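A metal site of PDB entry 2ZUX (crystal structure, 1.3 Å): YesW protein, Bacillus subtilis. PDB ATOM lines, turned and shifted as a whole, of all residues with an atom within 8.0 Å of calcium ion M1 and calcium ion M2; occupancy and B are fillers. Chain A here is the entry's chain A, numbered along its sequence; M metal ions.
Calcium ion M1 is bound by the side-chain carboxylate (OD1) of Asp 349, 2.4 Å away. The side-chain carboxylate (OE2) of Glu 340 binds calcium ion M1 (2.4 Å). The side-chain carboxylate (OD2) of Asp 336 binds calcium ion M1 (2.4 Å). OD2 of Asp 334 binds calcium ion M1. A ring nitrogen (ND1) of His 350 binds calcium ion M1, at 2.6 Å. Calcium ion M1 has five donor atoms within binding distance.
OD1 of Asp 336 is bound to calcium ion M2, 2.1 Å away. Calcium ion M2 is bound by the side-chain carboxylate (OD1) of Asp 334, at 2.1 Å. Calcium ion M2 is bound by O of Lys 338 (2.2 Å). OE2 of Glu 340 binds calcium ion M2, 2.3 Å away. Calcium ion M2 is bound by OD1 of Asp 332. OE1 of Glu 340 is bound to calcium ion M2 (2.4 Å).
The nearest printed residue that does not touch calcium ion M2 is Val 333 (4.1 Å).
N of Asp 349 sits close to SD of Met 355, 3.5 Å away. The backbone NH of Gly 337 sits at hydrogen-bond distance from the side-chain carboxylate of Asp 332 (2.8 Å). The side-chain carboxylate (OE1) of Glu 340 sits close to the backbone NH (N) of Val 333, 2.9 Å away. The side-chain carboxylate of Asp 339 lies within hydrogen-bond range of the backbone NH of Asp 332. The backbone NH (N) of Glu 340 sits at hydrogen-bond distance from the backbone carbonyl oxygen (O) of Ala 331, 2.8 Å away. OD1 of Asp 332 lies close to N of Gly 335.
Of the 20 residues printed, 5 come within 4 Å of calcium ion M1.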
ATOM      1  N   ARG A   3     -17.659  16.815 -14.501  1.00  0.00           N
ATOM      2  CA  ARG A   3     -18.373  18.024 -14.949  1.00  0.00           C
ATOM      3  C   ARG A   3     -18.073  19.226 -14.080  1.00  0.00           C
ATOM      4  O   ARG A   3     -17.972  19.108 -12.854  1.00  0.00           O
ATOM      5  CB  ARG A   3     -19.886  17.807 -14.882  1.00  0.00           C
ATOM      6  CG  ARG A   3     -20.428  16.878 -15.891  1.00  0.00           C
ATOM      7  CD  ARG A   3     -21.933  16.965 -15.908  1.00  0.00           C
ATOM      8  NE  ARG A   3     -22.444  16.152 -16.983  1.00  0.00           N
ATOM      9  CZ  ARG A   3     -23.592  16.374 -17.601  1.00  0.00           C
ATOM     10  NH1 ARG A   3     -24.375  17.379 -17.237  1.00  0.00           N
ATOM     11  NH2 ARG A   3     -23.945  15.571 -18.585  1.00  0.00           N
ATOM     12  N   TYR A 274     -24.742  20.265 -20.927  1.00  0.00           N
ATOM     13  CA  TYR A 274     -23.316  19.956 -21.049  1.00  0.00           C
ATOM     14  C   TYR A 274     -23.105  19.109 -22.308  1.00  0.00           C
ATOM     15  O   TYR A 274     -22.898  17.886 -22.234  1.00  0.00           O
ATOM     16  CB  TYR A 274     -22.806  19.235 -19.794  1.00  0.00           C
ATOM     17  CG  TYR A 274     -22.634  20.138 -18.586  1.00  0.00           C
ATOM     18  CD1 TYR A 274     -21.408  20.204 -17.914  1.00  0.00           C
ATOM     19  CD2 TYR A 274     -23.684  20.940 -18.128  1.00  0.00           C
ATOM     20  CE1 TYR A 274     -21.247  21.038 -16.807  1.00  0.00           C
ATOM     21  CE2 TYR A 274     -23.527  21.770 -17.013  1.00  0.00           C
ATOM     22  CZ  TYR A 274     -22.303  21.814 -16.365  1.00  0.00           C
ATOM     23  OH  TYR A 274     -22.143  22.634 -15.279  1.00  0.00           O
ATOM     24  N   LEU A 275     -23.163  19.774 -23.457  1.00  0.00           N
ATOM     25  CA  LEU A 275     -23.081  19.113 -24.749  1.00  0.00           C
ATOM     26  C   LEU A 275     -21.741  18.435 -24.994  1.00  0.00           C
ATOM     27  O   LEU A 275     -21.673  17.420 -25.710  1.00  0.00           O
ATOM     28  CB  LEU A 275     -23.375  20.103 -25.872  1.00  0.00           C
ATOM     29  CG  LEU A 275     -24.721  20.847 -25.764  1.00  0.00           C
ATOM     30  CD1 LEU A 275     -24.781  21.944 -26.805  1.00  0.00           C
ATOM     31  CD2 LEU A 275     -25.896  19.888 -25.904  1.00  0.00           C
ATOM     32  N   GLY A 277     -19.931  17.266 -22.420  1.00  0.00           N
ATOM     33  CA  GLY A 277     -19.765  16.340 -21.298  1.00  0.00           C
ATOM     34  C   GLY A 277     -18.949  16.875 -20.135  1.00  0.00           C
ATOM     35  O   GLY A 277     -18.764  16.175 -19.137  1.00  0.00           O
ATOM     36  N   ALA A 331     -30.691  15.948 -19.981  1.00  0.00           N
ATOM     37  CA  ALA A 331     -30.091  14.847 -19.263  1.00  0.00           C
ATOM     38  C   ALA A 331     -29.204  14.046 -20.191  1.00  0.00           C
ATOM     39  O   ALA A 331     -29.445  13.982 -21.398  1.00  0.00           O
ATOM     40  CB  ALA A 331     -31.162  13.927 -18.674  1.00  0.00           C
ATOM     41  N   ASP A 332     -28.208  13.385 -19.617  1.00  0.00           N
ATOM     42  CA  ASP A 332     -27.438  12.401 -20.360  1.00  0.00           C
ATOM     43  C   ASP A 332     -28.260  11.117 -20.365  1.00  0.00           C
ATOM     44  O   ASP A 332     -28.297  10.386 -19.369  1.00  0.00           O
ATOM     45  CB  ASP A 332     -26.072  12.179 -19.720  1.00  0.00           C
ATOM     46  CG  ASP A 332     -25.279  11.072 -20.392  1.00  0.00           C
ATOM     47  OD1 ASP A 332     -25.612  10.692 -21.535  1.00  0.00           O
ATOM     48  OD2 ASP A 332     -24.318  10.575 -19.777  1.00  0.00           O
ATOM     49  N   VAL A 333     -28.925  10.859 -21.484  1.00  0.00           N
ATOM     50  CA  VAL A 333     -29.837   9.722 -21.578  1.00  0.00           C
ATOM     51  C   VAL A 333     -29.177   8.491 -22.188  1.00  0.00           C
ATOM     52  O   VAL A 333     -29.636   7.379 -21.974  1.00  0.00           O
ATOM     53  CB  VAL A 333     -31.128  10.052 -22.388  1.00  0.00           C
ATOM     54  CG1 VAL A 333     -31.871  11.237 -21.764  1.00  0.00           C
ATOM     55  CG2 VAL A 333     -30.806  10.315 -23.877  1.00  0.00           C
ATOM     56  N   ASP A 334     -28.104   8.692 -22.955  1.00  0.00           N
ATOM     57  CA  ASP A 334     -27.486   7.600 -23.704  1.00  0.00           C
ATOM     58  C   ASP A 334     -26.169   7.109 -23.104  1.00  0.00           C
ATOM     59  O   ASP A 334     -25.537   6.195 -23.648  1.00  0.00           O
ATOM     60  CB  ASP A 334     -27.345   7.958 -25.199  1.00  0.00           C
ATOM     61  CG  ASP A 334     -26.492   9.197 -25.424  1.00  0.00           C
ATOM     62  OD1 ASP A 334     -25.833   9.642 -24.476  1.00  0.00           O
ATOM     63  OD2 ASP A 334     -26.494   9.722 -26.565  1.00  0.00           O
ATOM     64  N   GLY A 335     -25.756   7.702 -21.989  1.00  0.00           N
ATOM     65  CA  GLY A 335     -24.604   7.243 -21.212  1.00  0.00           C
ATOM     66  C   GLY A 335     -23.236   7.678 -21.687  1.00  0.00           C
ATOM     67  O   GLY A 335     -22.223   7.157 -21.190  1.00  0.00           O
ATOM     68  N   ASP A 336     -23.165   8.617 -22.629  1.00  0.00           N
ATOM     69  CA  ASP A 336     -21.880   9.085 -23.153  1.00  0.00           C
ATOM     70  C   ASP A 336     -21.275  10.259 -22.360  1.00  0.00           C
ATOM     71  O   ASP A 336     -20.222  10.800 -22.743  1.00  0.00           O
ATOM     72  CB  ASP A 336     -21.979   9.414 -24.660  1.00  0.00           C
ATOM     73  CG  ASP A 336     -22.939  10.559 -24.976  1.00  0.00           C
ATOM     74  OD1 ASP A 336     -23.399  11.234 -24.016  1.00  0.00           O
ATOM     75  OD2 ASP A 336     -23.258  10.792 -26.158  1.00  0.00           O
ATOM     76  N   GLY A 337     -21.928  10.657 -21.269  1.00  0.00           N
ATOM     77  CA  GLY A 337     -21.468  11.763 -20.420  1.00  0.00           C
ATOM     78  C   GLY A 337     -21.953  13.133 -20.866  1.00  0.00           C
ATOM     79  O   GLY A 337     -21.864  14.120 -20.128  1.00  0.00           O
ATOM     80  N   LYS A 338     -22.461  13.180 -22.088  1.00  0.00           N
ATOM     81  CA  LYS A 338     -22.899  14.418 -22.730  1.00  0.00           C
ATOM     82  C   LYS A 338     -24.415  14.536 -22.638  1.00  0.00           C
ATOM     83  O   LYS A 338     -25.130  13.541 -22.721  1.00  0.00           O
ATOM     84  CB  LYS A 338     -22.459  14.428 -24.185  1.00  0.00           C
ATOM     85  CG  LYS A 338     -20.951  14.228 -24.345  1.00  0.00           C
ATOM     86  CD  LYS A 338     -20.544  14.181 -25.797  1.00  0.00           C
ATOM     87  CE  LYS A 338     -19.038  13.982 -25.932  1.00  0.00           C
ATOM     88  NZ  LYS A 338     -18.618  12.621 -25.472  1.00  0.00           N
ATOM     89  N   ASP A 339     -24.912  15.762 -22.462  1.00  0.00           N
ATOM     90  CA  ASP A 339     -26.352  15.974 -22.317  1.00  0.00           C
ATOM     91  C   ASP A 339     -27.101  15.983 -23.631  1.00  0.00           C
ATOM     92  O   ASP A 339     -26.660  16.554 -24.624  1.00  0.00           O
ATOM     93  CB  ASP A 339     -26.628  17.282 -21.570  1.00  0.00           C
ATOM     94  CG  ASP A 339     -26.310  17.204 -20.102  1.00  0.00           C
ATOM     95  OD1 ASP A 339     -26.409  16.095 -19.521  1.00  0.00           O
ATOM     96  OD2 ASP A 339     -25.941  18.237 -19.521  1.00  0.00           O
ATOM     97  N   GLU A 340     -28.254  15.322 -23.594  1.00  0.00           N
ATOM     98  CA  GLU A 340     -29.244  15.390 -24.652  1.00  0.00           C
ATOM     99  C   GLU A 340     -30.411  16.251 -24.177  1.00  0.00           C
ATOM    100  O   GLU A 340     -30.511  16.596 -22.991  1.00  0.00           O
ATOM    101  CB  GLU A 340     -29.705  13.973 -24.999  1.00  0.00           C
ATOM    102  CG  GLU A 340     -28.671  13.158 -25.803  1.00  0.00           C
ATOM    103  CD  GLU A 340     -27.517  12.623 -24.945  1.00  0.00           C
ATOM    104  OE1 GLU A 340     -27.758  12.124 -23.818  1.00  0.00           O
ATOM    105  OE2 GLU A 340     -26.330  12.714 -25.388  1.00  0.00           O
ATOM    106  N   ILE A 341     -31.278  16.606 -25.115  1.00  0.00           N
ATOM    107  CA  ILE A 341     -32.403  17.501 -24.850  1.00  0.00           C
ATOM    108  C   ILE A 341     -33.702  16.727 -25.072  1.00  0.00           C
ATOM    109  O   ILE A 341     -33.922  16.187 -26.168  1.00  0.00           O
ATOM    110  CB  ILE A 341     -32.367  18.726 -25.784  1.00  0.00           C
ATOM    111  CG1 ILE A 341     -31.050  19.511 -25.611  1.00  0.00           C
ATOM    112  CG2 ILE A 341     -33.571  19.633 -25.539  1.00  0.00           C
ATOM    113  CD1 ILE A 341     -30.625  20.310 -26.826  1.00  0.00           C
ATOM    114  N   VAL A 348     -33.213  15.495 -28.906  1.00  0.00           N
ATOM    115  CA  VAL A 348     -32.137  16.029 -29.720  1.00  0.00           C
ATOM    116  C   VAL A 348     -30.827  15.653 -29.059  1.00  0.00           C
ATOM    117  O   VAL A 348     -30.667  15.807 -27.850  1.00  0.00           O
ATOM    118  CB  VAL A 348     -32.258  17.564 -29.849  1.00  0.00           C
ATOM    119  CG1 VAL A 348     -31.124  18.158 -30.690  1.00  0.00           C
ATOM    120  CG2 VAL A 348     -33.615  17.945 -30.424  1.00  0.00           C
ATOM    121  N   ASP A 349     -29.894  15.146 -29.874  1.00  0.00           N
ATOM    122  CA  ASP A 349     -28.592  14.687 -29.383  1.00  0.00           C
ATOM    123  C   ASP A 349     -27.681  15.861 -29.031  1.00  0.00           C
ATOM    124  O   ASP A 349     -27.959  17.007 -29.386  1.00  0.00           O
ATOM    125  CB  ASP A 349     -27.954  13.789 -30.447  1.00  0.00           C
ATOM    126  CG  ASP A 349     -27.060  12.718 -29.874  1.00  0.00           C
ATOM    127  OD1 ASP A 349     -26.810  12.677 -28.646  1.00  0.00           O
ATOM    128  OD2 ASP A 349     -26.591  11.886 -30.684  1.00  0.00           O
ATOM    129  N   HIS A 350     -26.568  15.545 -28.376  1.00  0.00           N
ATOM    130  CA  HIS A 350     -25.636  16.560 -27.895  1.00  0.00           C
ATOM    131  C   HIS A 350     -25.002  17.367 -29.026  1.00  0.00           C
ATOM    132  O   HIS A 350     -24.477  18.455 -28.791  1.00  0.00           O
ATOM    133  CB  HIS A 350     -24.545  15.899 -27.059  1.00  0.00           C
ATOM    134  CG  HIS A 350     -23.603  15.047 -27.849  1.00  0.00           C
ATOM    135  ND1 HIS A 350     -23.770  13.690 -28.008  1.00  0.00           N
ATOM    136  CD2 HIS A 350     -22.497  15.371 -28.564  1.00  0.00           C
ATOM    137  CE1 HIS A 350     -22.802  13.210 -28.775  1.00  0.00           C
ATOM    138  NE2 HIS A 350     -22.017  14.222 -29.122  1.00  0.00           N
ATOM    139  N   ASP A 351     -25.036  16.828 -30.246  1.00  0.00           N
ATOM    140  CA  ASP A 351     -24.488  17.475 -31.429  1.00  0.00           C
ATOM    141  C   ASP A 351     -25.559  18.141 -32.300  1.00  0.00           C
ATOM    142  O   ASP A 351     -25.282  18.567 -33.426  1.00  0.00           O
ATOM    143  CB  ASP A 351     -23.696  16.464 -32.260  1.00  0.00           C
ATOM    144  CG  ASP A 351     -24.556  15.329 -32.777  1.00  0.00           C
ATOM    145  OD1 ASP A 351     -25.757  15.243 -32.430  1.00  0.00           O
ATOM    146  OD2 ASP A 351     -24.031  14.495 -33.541  1.00  0.00           O
ATOM    147  N   MET A 355     -32.855  12.803 -32.556  1.00  0.00           N
ATOM    148  CA  MET A 355     -32.706  11.400 -32.159  1.00  0.00           C
ATOM    149  C   MET A 355     -33.933  10.545 -32.486  1.00  0.00           C
ATOM    150  O   MET A 355     -33.822   9.486 -33.107  1.00  0.00           O
ATOM    151  CB  MET A 355     -32.419  11.278 -30.667  1.00  0.00           C
ATOM    152  CG  MET A 355     -31.093  11.885 -30.265  1.00  0.00           C
ATOM    153  SD  MET A 355     -30.916  12.078 -28.481  1.00  0.00           S
ATOM    154  CE  MET A 355     -30.849  10.379 -27.929  1.00  0.00           C
HETATM  155 CA    CA M   1     -25.221  11.700 -27.212  1.00  0.00          CA
HETATM  156 CA    CA M   2     -25.464  11.575 -23.633  1.00  0.00          CA
